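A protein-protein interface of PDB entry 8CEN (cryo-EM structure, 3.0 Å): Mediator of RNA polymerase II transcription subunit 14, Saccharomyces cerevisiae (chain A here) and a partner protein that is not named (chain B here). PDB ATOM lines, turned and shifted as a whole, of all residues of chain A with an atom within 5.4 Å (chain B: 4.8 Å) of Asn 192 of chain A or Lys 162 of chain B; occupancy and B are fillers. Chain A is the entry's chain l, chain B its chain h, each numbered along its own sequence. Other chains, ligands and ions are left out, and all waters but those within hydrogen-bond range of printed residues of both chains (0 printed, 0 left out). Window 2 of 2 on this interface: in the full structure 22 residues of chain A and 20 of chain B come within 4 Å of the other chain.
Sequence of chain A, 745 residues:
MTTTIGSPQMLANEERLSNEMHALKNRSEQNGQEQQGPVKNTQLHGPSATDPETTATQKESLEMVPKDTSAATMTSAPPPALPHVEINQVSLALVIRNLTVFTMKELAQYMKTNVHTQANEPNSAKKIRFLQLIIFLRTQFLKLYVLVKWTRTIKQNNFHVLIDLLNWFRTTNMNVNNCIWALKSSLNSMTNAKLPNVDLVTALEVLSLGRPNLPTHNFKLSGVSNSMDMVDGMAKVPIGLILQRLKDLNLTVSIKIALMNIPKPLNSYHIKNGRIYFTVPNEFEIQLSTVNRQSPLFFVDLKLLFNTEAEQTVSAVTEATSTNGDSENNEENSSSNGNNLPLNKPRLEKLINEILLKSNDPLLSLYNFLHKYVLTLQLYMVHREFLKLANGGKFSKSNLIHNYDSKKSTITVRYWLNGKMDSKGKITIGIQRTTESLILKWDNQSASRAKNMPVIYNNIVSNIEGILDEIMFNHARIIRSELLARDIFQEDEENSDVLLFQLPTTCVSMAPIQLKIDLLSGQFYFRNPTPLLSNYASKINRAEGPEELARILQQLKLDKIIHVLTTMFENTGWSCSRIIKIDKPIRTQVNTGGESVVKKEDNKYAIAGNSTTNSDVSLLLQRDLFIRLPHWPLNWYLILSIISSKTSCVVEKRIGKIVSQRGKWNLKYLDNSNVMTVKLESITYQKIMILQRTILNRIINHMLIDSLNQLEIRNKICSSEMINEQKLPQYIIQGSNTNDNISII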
ATOM      1  N   ASN A 188     -15.397 -14.078   8.698  1.00  0.00           N
ATOM      2  CA  ASN A 188     -16.499 -13.888   7.762  1.00  0.00           C
ATOM      3  C   ASN A 188     -17.061 -12.476   7.811  1.00  0.00           C
ATOM      4  O   ASN A 188     -17.674 -12.031   6.835  1.00  0.00           O
ATOM      5  CB  ASN A 188     -17.609 -14.902   8.040  1.00  0.00           C
ATOM      6  CG  ASN A 188     -17.130 -16.332   7.914  1.00  0.00           C
ATOM      7  OD1 ASN A 188     -16.342 -16.658   7.027  1.00  0.00           O
ATOM      8  ND2 ASN A 188     -17.607 -17.198   8.802  1.00  0.00           N
ATOM      9  N   SER A 189     -16.866 -11.769   8.925  1.00  0.00           N
ATOM     10  CA  SER A 189     -17.250 -10.365   9.010  1.00  0.00           C
ATOM     11  C   SER A 189     -16.400  -9.468   8.119  1.00  0.00           C
ATOM     12  O   SER A 189     -16.809  -8.339   7.829  1.00  0.00           O
ATOM     13  CB  SER A 189     -17.148  -9.888  10.458  1.00  0.00           C
ATOM     14  OG  SER A 189     -17.463  -8.511  10.563  1.00  0.00           O
ATOM     15  N   MET A 190     -15.236  -9.941   7.679  1.00  0.00           N
ATOM     16  CA  MET A 190     -14.272  -9.114   6.969  1.00  0.00           C
ATOM     17  C   MET A 190     -14.446  -9.156   5.457  1.00  0.00           C
ATOM     18  O   MET A 190     -13.709  -8.462   4.750  1.00  0.00           O
ATOM     19  CB  MET A 190     -12.855  -9.561   7.323  1.00  0.00           C
ATOM     20  CG  MET A 190     -12.537  -9.350   8.774  1.00  0.00           C
ATOM     21  SD  MET A 190     -12.541  -7.647   9.323  1.00  0.00           S
ATOM     22  CE  MET A 190     -12.374  -7.954  11.071  1.00  0.00           C
ATOM     23  N   THR A 191     -15.385  -9.959   4.949  1.00  0.00           N
ATOM     24  CA  THR A 191     -15.496 -10.159   3.507  1.00  0.00           C
ATOM     25  C   THR A 191     -15.978  -8.894   2.806  1.00  0.00           C
ATOM     26  O   THR A 191     -15.418  -8.488   1.781  1.00  0.00           O
ATOM     27  CB  THR A 191     -16.434 -11.332   3.212  1.00  0.00           C
ATOM     28  OG1 THR A 191     -17.743 -11.045   3.716  1.00  0.00           O
ATOM     29  CG2 THR A 191     -15.917 -12.593   3.881  1.00  0.00           C
ATOM     30  N   ASN A 192     -17.008  -8.251   3.350  1.00  0.00           N
ATOM     31  CA  ASN A 192     -17.496  -7.010   2.770  1.00  0.00           C
ATOM     32  C   ASN A 192     -16.602  -5.824   3.113  1.00  0.00           C
ATOM     33  O   ASN A 192     -16.608  -4.823   2.387  1.00  0.00           O
ATOM     34  CB  ASN A 192     -18.932  -6.760   3.245  1.00  0.00           C
ATOM     35  CG  ASN A 192     -19.510  -5.459   2.725  1.00  0.00           C
ATOM     36  OD1 ASN A 192     -20.264  -4.784   3.422  1.00  0.00           O
ATOM     37  ND2 ASN A 192     -19.182  -5.115   1.484  1.00  0.00           N
ATOM     38  N   ALA A 193     -15.790  -5.930   4.160  1.00  0.00           N
ATOM     39  CA  ALA A 193     -15.069  -4.785   4.703  1.00  0.00           C
ATOM     40  C   ALA A 193     -13.656  -4.770   4.133  1.00  0.00           C
ATOM     41  O   ALA A 193     -12.688  -5.154   4.789  1.00  0.00           O
ATOM     42  CB  ALA A 193     -15.055  -4.852   6.196  1.00  0.00           C
ATOM     43  N   LYS A 194     -13.549  -4.307   2.891  1.00  0.00           N
ATOM     44  CA  LYS A 194     -12.287  -3.963   2.252  1.00  0.00           C
ATOM     45  C   LYS A 194     -12.521  -2.701   1.435  1.00  0.00           C
ATOM     46  O   LYS A 194     -13.583  -2.074   1.508  1.00  0.00           O
ATOM     47  CB  LYS A 194     -11.744  -5.091   1.358  1.00  0.00           C
ATOM     48  CG  LYS A 194     -11.700  -6.483   1.963  1.00  0.00           C
ATOM     49  CD  LYS A 194     -10.396  -6.702   2.707  1.00  0.00           C
ATOM     50  CE  LYS A 194     -10.567  -7.702   3.835  1.00  0.00           C
ATOM     51  NZ  LYS A 194     -11.047  -9.019   3.351  1.00  0.00           N
ATOM     52  N   LEU A 195     -11.527  -2.333   0.647  1.00  0.00           N
ATOM     53  CA  LEU A 195     -11.687  -1.288  -0.351  1.00  0.00           C
ATOM     54  C   LEU A 195     -10.799  -1.663  -1.527  1.00  0.00           C
ATOM     55  O   LEU A 195      -9.570  -1.570  -1.430  1.00  0.00           O
ATOM     56  CB  LEU A 195     -11.328   0.083   0.216  1.00  0.00           C
ATOM     57  CG  LEU A 195     -12.029   1.289  -0.409  1.00  0.00           C
ATOM     58  CD1 LEU A 195     -13.533   1.085  -0.412  1.00  0.00           C
ATOM     59  CD2 LEU A 195     -11.669   2.556   0.344  1.00  0.00           C
ATOM     60  N   PRO A 196     -11.382  -2.108  -2.644  1.00  0.00           N
ATOM     61  CA  PRO A 196     -10.578  -2.720  -3.711  1.00  0.00           C
ATOM     62  C   PRO A 196      -9.701  -1.736  -4.464  1.00  0.00           C
ATOM     63  O   PRO A 196      -9.715  -0.532  -4.193  1.00  0.00           O
ATOM     64  CB  PRO A 196     -11.638  -3.332  -4.638  1.00  0.00           C
ATOM     65  CG  PRO A 196     -12.882  -3.418  -3.807  1.00  0.00           C
ATOM     66  CD  PRO A 196     -12.823  -2.228  -2.910  1.00  0.00           C
ATOM     67  N   LYS B 159     -15.586   4.986  -6.896  1.00  0.00           N
ATOM     68  CA  LYS B 159     -16.936   4.429  -6.906  1.00  0.00           C
ATOM     69  C   LYS B 159     -16.962   3.078  -7.611  1.00  0.00           C
ATOM     70  O   LYS B 159     -17.575   2.121  -7.120  1.00  0.00           O
ATOM     71  CB  LYS B 159     -17.905   5.398  -7.579  1.00  0.00           C
ATOM     72  CG  LYS B 159     -18.374   6.529  -6.694  1.00  0.00           C
ATOM     73  CD  LYS B 159     -19.503   7.294  -7.354  1.00  0.00           C
ATOM     74  CE  LYS B 159     -19.824   8.562  -6.589  1.00  0.00           C
ATOM     75  NZ  LYS B 159     -20.927   9.331  -7.233  1.00  0.00           N
ATOM     76  N   LEU B 160     -16.299   2.981  -8.764  1.00  0.00           N
ATOM     77  CA  LEU B 160     -16.312   1.754  -9.553  1.00  0.00           C
ATOM     78  C   LEU B 160     -15.349   0.688  -9.047  1.00  0.00           C
ATOM     79  O   LEU B 160     -15.326  -0.408  -9.619  1.00  0.00           O
ATOM     80  CB  LEU B 160     -15.976   2.052 -11.015  1.00  0.00           C
ATOM     81  CG  LEU B 160     -16.881   3.007 -11.785  1.00  0.00           C
ATOM     82  CD1 LEU B 160     -16.350   3.172 -13.192  1.00  0.00           C
ATOM     83  CD2 LEU B 160     -18.309   2.502 -11.799  1.00  0.00           C
ATOM     84  N   SER B 161     -14.536   0.997  -8.033  1.00  0.00           N
ATOM     85  CA  SER B 161     -13.544   0.042  -7.539  1.00  0.00           C
ATOM     86  C   SER B 161     -14.185  -1.240  -7.015  1.00  0.00           C
ATOM     87  O   SER B 161     -13.677  -2.340  -7.264  1.00  0.00           O
ATOM     88  CB  SER B 161     -12.697   0.692  -6.447  1.00  0.00           C
ATOM     89  OG  SER B 161     -13.511   1.170  -5.390  1.00  0.00           O
ATOM     90  N   LYS B 162     -15.296  -1.126  -6.296  1.00  0.00           N
ATOM     91  CA  LYS B 162     -15.920  -2.288  -5.680  1.00  0.00           C
ATOM     92  C   LYS B 162     -16.863  -3.034  -6.616  1.00  0.00           C
ATOM     93  O   LYS B 162     -17.437  -4.049  -6.210  1.00  0.00           O
ATOM     94  CB  LYS B 162     -16.681  -1.873  -4.416  1.00  0.00           C
ATOM     95  CG  LYS B 162     -16.570  -2.875  -3.278  1.00  0.00           C
ATOM     96  CD  LYS B 162     -17.657  -2.669  -2.240  1.00  0.00           C
ATOM     97  CE  LYS B 162     -17.177  -1.781  -1.108  1.00  0.00           C
ATOM     98  NZ  LYS B 162     -18.128  -1.795   0.037  1.00  0.00           N
ATOM     99  N   PHE B 163     -17.035  -2.572  -7.852  1.00  0.00           N
ATOM    100  CA  PHE B 163     -18.020  -3.155  -8.753  1.00  0.00           C
ATOM    101  C   PHE B 163     -17.410  -3.758 -10.008  1.00  0.00           C
ATOM    102  O   PHE B 163     -17.700  -4.913 -10.338  1.00  0.00           O
ATOM    103  CB  PHE B 163     -19.062  -2.094  -9.131  1.00  0.00           C
ATOM    104  CG  PHE B 163     -19.992  -1.743  -8.010  1.00  0.00           C
ATOM    105  CD1 PHE B 163     -21.117  -2.511  -7.762  1.00  0.00           C
ATOM    106  CD2 PHE B 163     -19.728  -0.661  -7.187  1.00  0.00           C
ATOM    107  CE1 PHE B 163     -21.972  -2.196  -6.728  1.00  0.00           C
ATOM    108  CE2 PHE B 163     -20.580  -0.342  -6.147  1.00  0.00           C
ATOM    109  CZ  PHE B 163     -21.703  -1.111  -5.917  1.00  0.00           C
ATOM    110  N   THR B 164     -16.560  -3.015 -10.715  1.00  0.00           N
ATOM    111  CA  THR B 164     -16.161  -3.400 -12.063  1.00  0.00           C
ATOM    112  C   THR B 164     -15.157  -4.547 -12.108  1.00  0.00           C
ATOM    113  O   THR B 164     -14.864  -5.035 -13.205  1.00  0.00           O
ATOM    114  CB  THR B 164     -15.595  -2.185 -12.794  1.00  0.00           C
ATOM    115  OG1 THR B 164     -14.500  -1.647 -12.046  1.00  0.00           O
ATOM    116  CG2 THR B 164     -16.663  -1.119 -12.954  1.00  0.00           C
ATOM    117  N   LYS B 165     -14.622  -4.989 -10.972  1.00  0.00           N
ATOM    118  CA  LYS B 165     -13.706  -6.120 -10.930  1.00  0.00           C
ATOM    119  C   LYS B 165     -14.122  -7.077  -9.820  1.00  0.00           C
ATOM    120  O   LYS B 165     -14.893  -6.722  -8.925  1.00  0.00           O
ATOM    121  CB  LYS B 165     -12.252  -5.675 -10.711  1.00  0.00           C
ATOM    122  CG  LYS B 165     -11.690  -4.775 -11.799  1.00  0.00           C
ATOM    123  CD  LYS B 165     -11.485  -5.537 -13.095  1.00  0.00           C
ATOM    124  CE  LYS B 165     -10.899  -4.642 -14.171  1.00  0.00           C
ATOM    125  NZ  LYS B 165      -9.507  -4.226 -13.844  1.00  0.00           N
ATOM    126  N   PHE B 180     -22.281  -7.150  -9.791  1.00  0.00           N
ATOM    127  CA  PHE B 180     -21.051  -6.411 -10.037  1.00  0.00           C
ATOM    128  C   PHE B 180     -21.042  -5.745 -11.406  1.00  0.00           C
ATOM    129  O   PHE B 180     -20.752  -4.552 -11.515  1.00  0.00           O
ATOM    130  CB  PHE B 180     -19.843  -7.344  -9.902  1.00  0.00           C
ATOM    131  CG  PHE B 180     -19.588  -7.811  -8.498  1.00  0.00           C
ATOM    132  CD1 PHE B 180     -20.277  -8.891  -7.974  1.00  0.00           C
ATOM    133  CD2 PHE B 180     -18.655  -7.169  -7.702  1.00  0.00           C
ATOM    134  CE1 PHE B 180     -20.043  -9.321  -6.686  1.00  0.00           C
ATOM    135  CE2 PHE B 180     -18.418  -7.595  -6.412  1.00  0.00           C
ATOM    136  CZ  PHE B 180     -19.110  -8.675  -5.905  1.00  0.00           C
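Of the 8 printed residues of chain B, 2 touch a printed residue of chain A. Among the printed residues, no Asp or Glu carboxylate lies within 4 Å of a Lys or Arg side-chain nitrogen of the other chain.
Asn 192 of chain A touches Lys 162 of chain B (ND2 to NZ, 3.8 Å). CB of Pro 196 of chain A touches O of Ser 161 of chain B (3.5 Å). Pro 196 of chain A touches Lys 162 of chain B.
Thr 191 of chain A touches none of the printed residues of chain B. Asn 192 of chain A touches just one residue of chain B: Lys 162. Of the printed residues of chain B, Pro 196 of chain A touches Ser 161 and Lys 162. Of the printed residues of chain A, Ser 161 of chain B touches Pro 196. Of chain A, only Asn 192 (3.8 Å) and Pro 196 (3.7 Å) come within 4 Å of Lys 162 of chain B. The nearest printed residue of chain B that does not touch Asn 192 of chain A is Phe 180 of chain B (8.2 Å). The nearest residue of chain A that does not touch Lys 162 of chain B is Lys 194 of chain A (4.5 Å).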
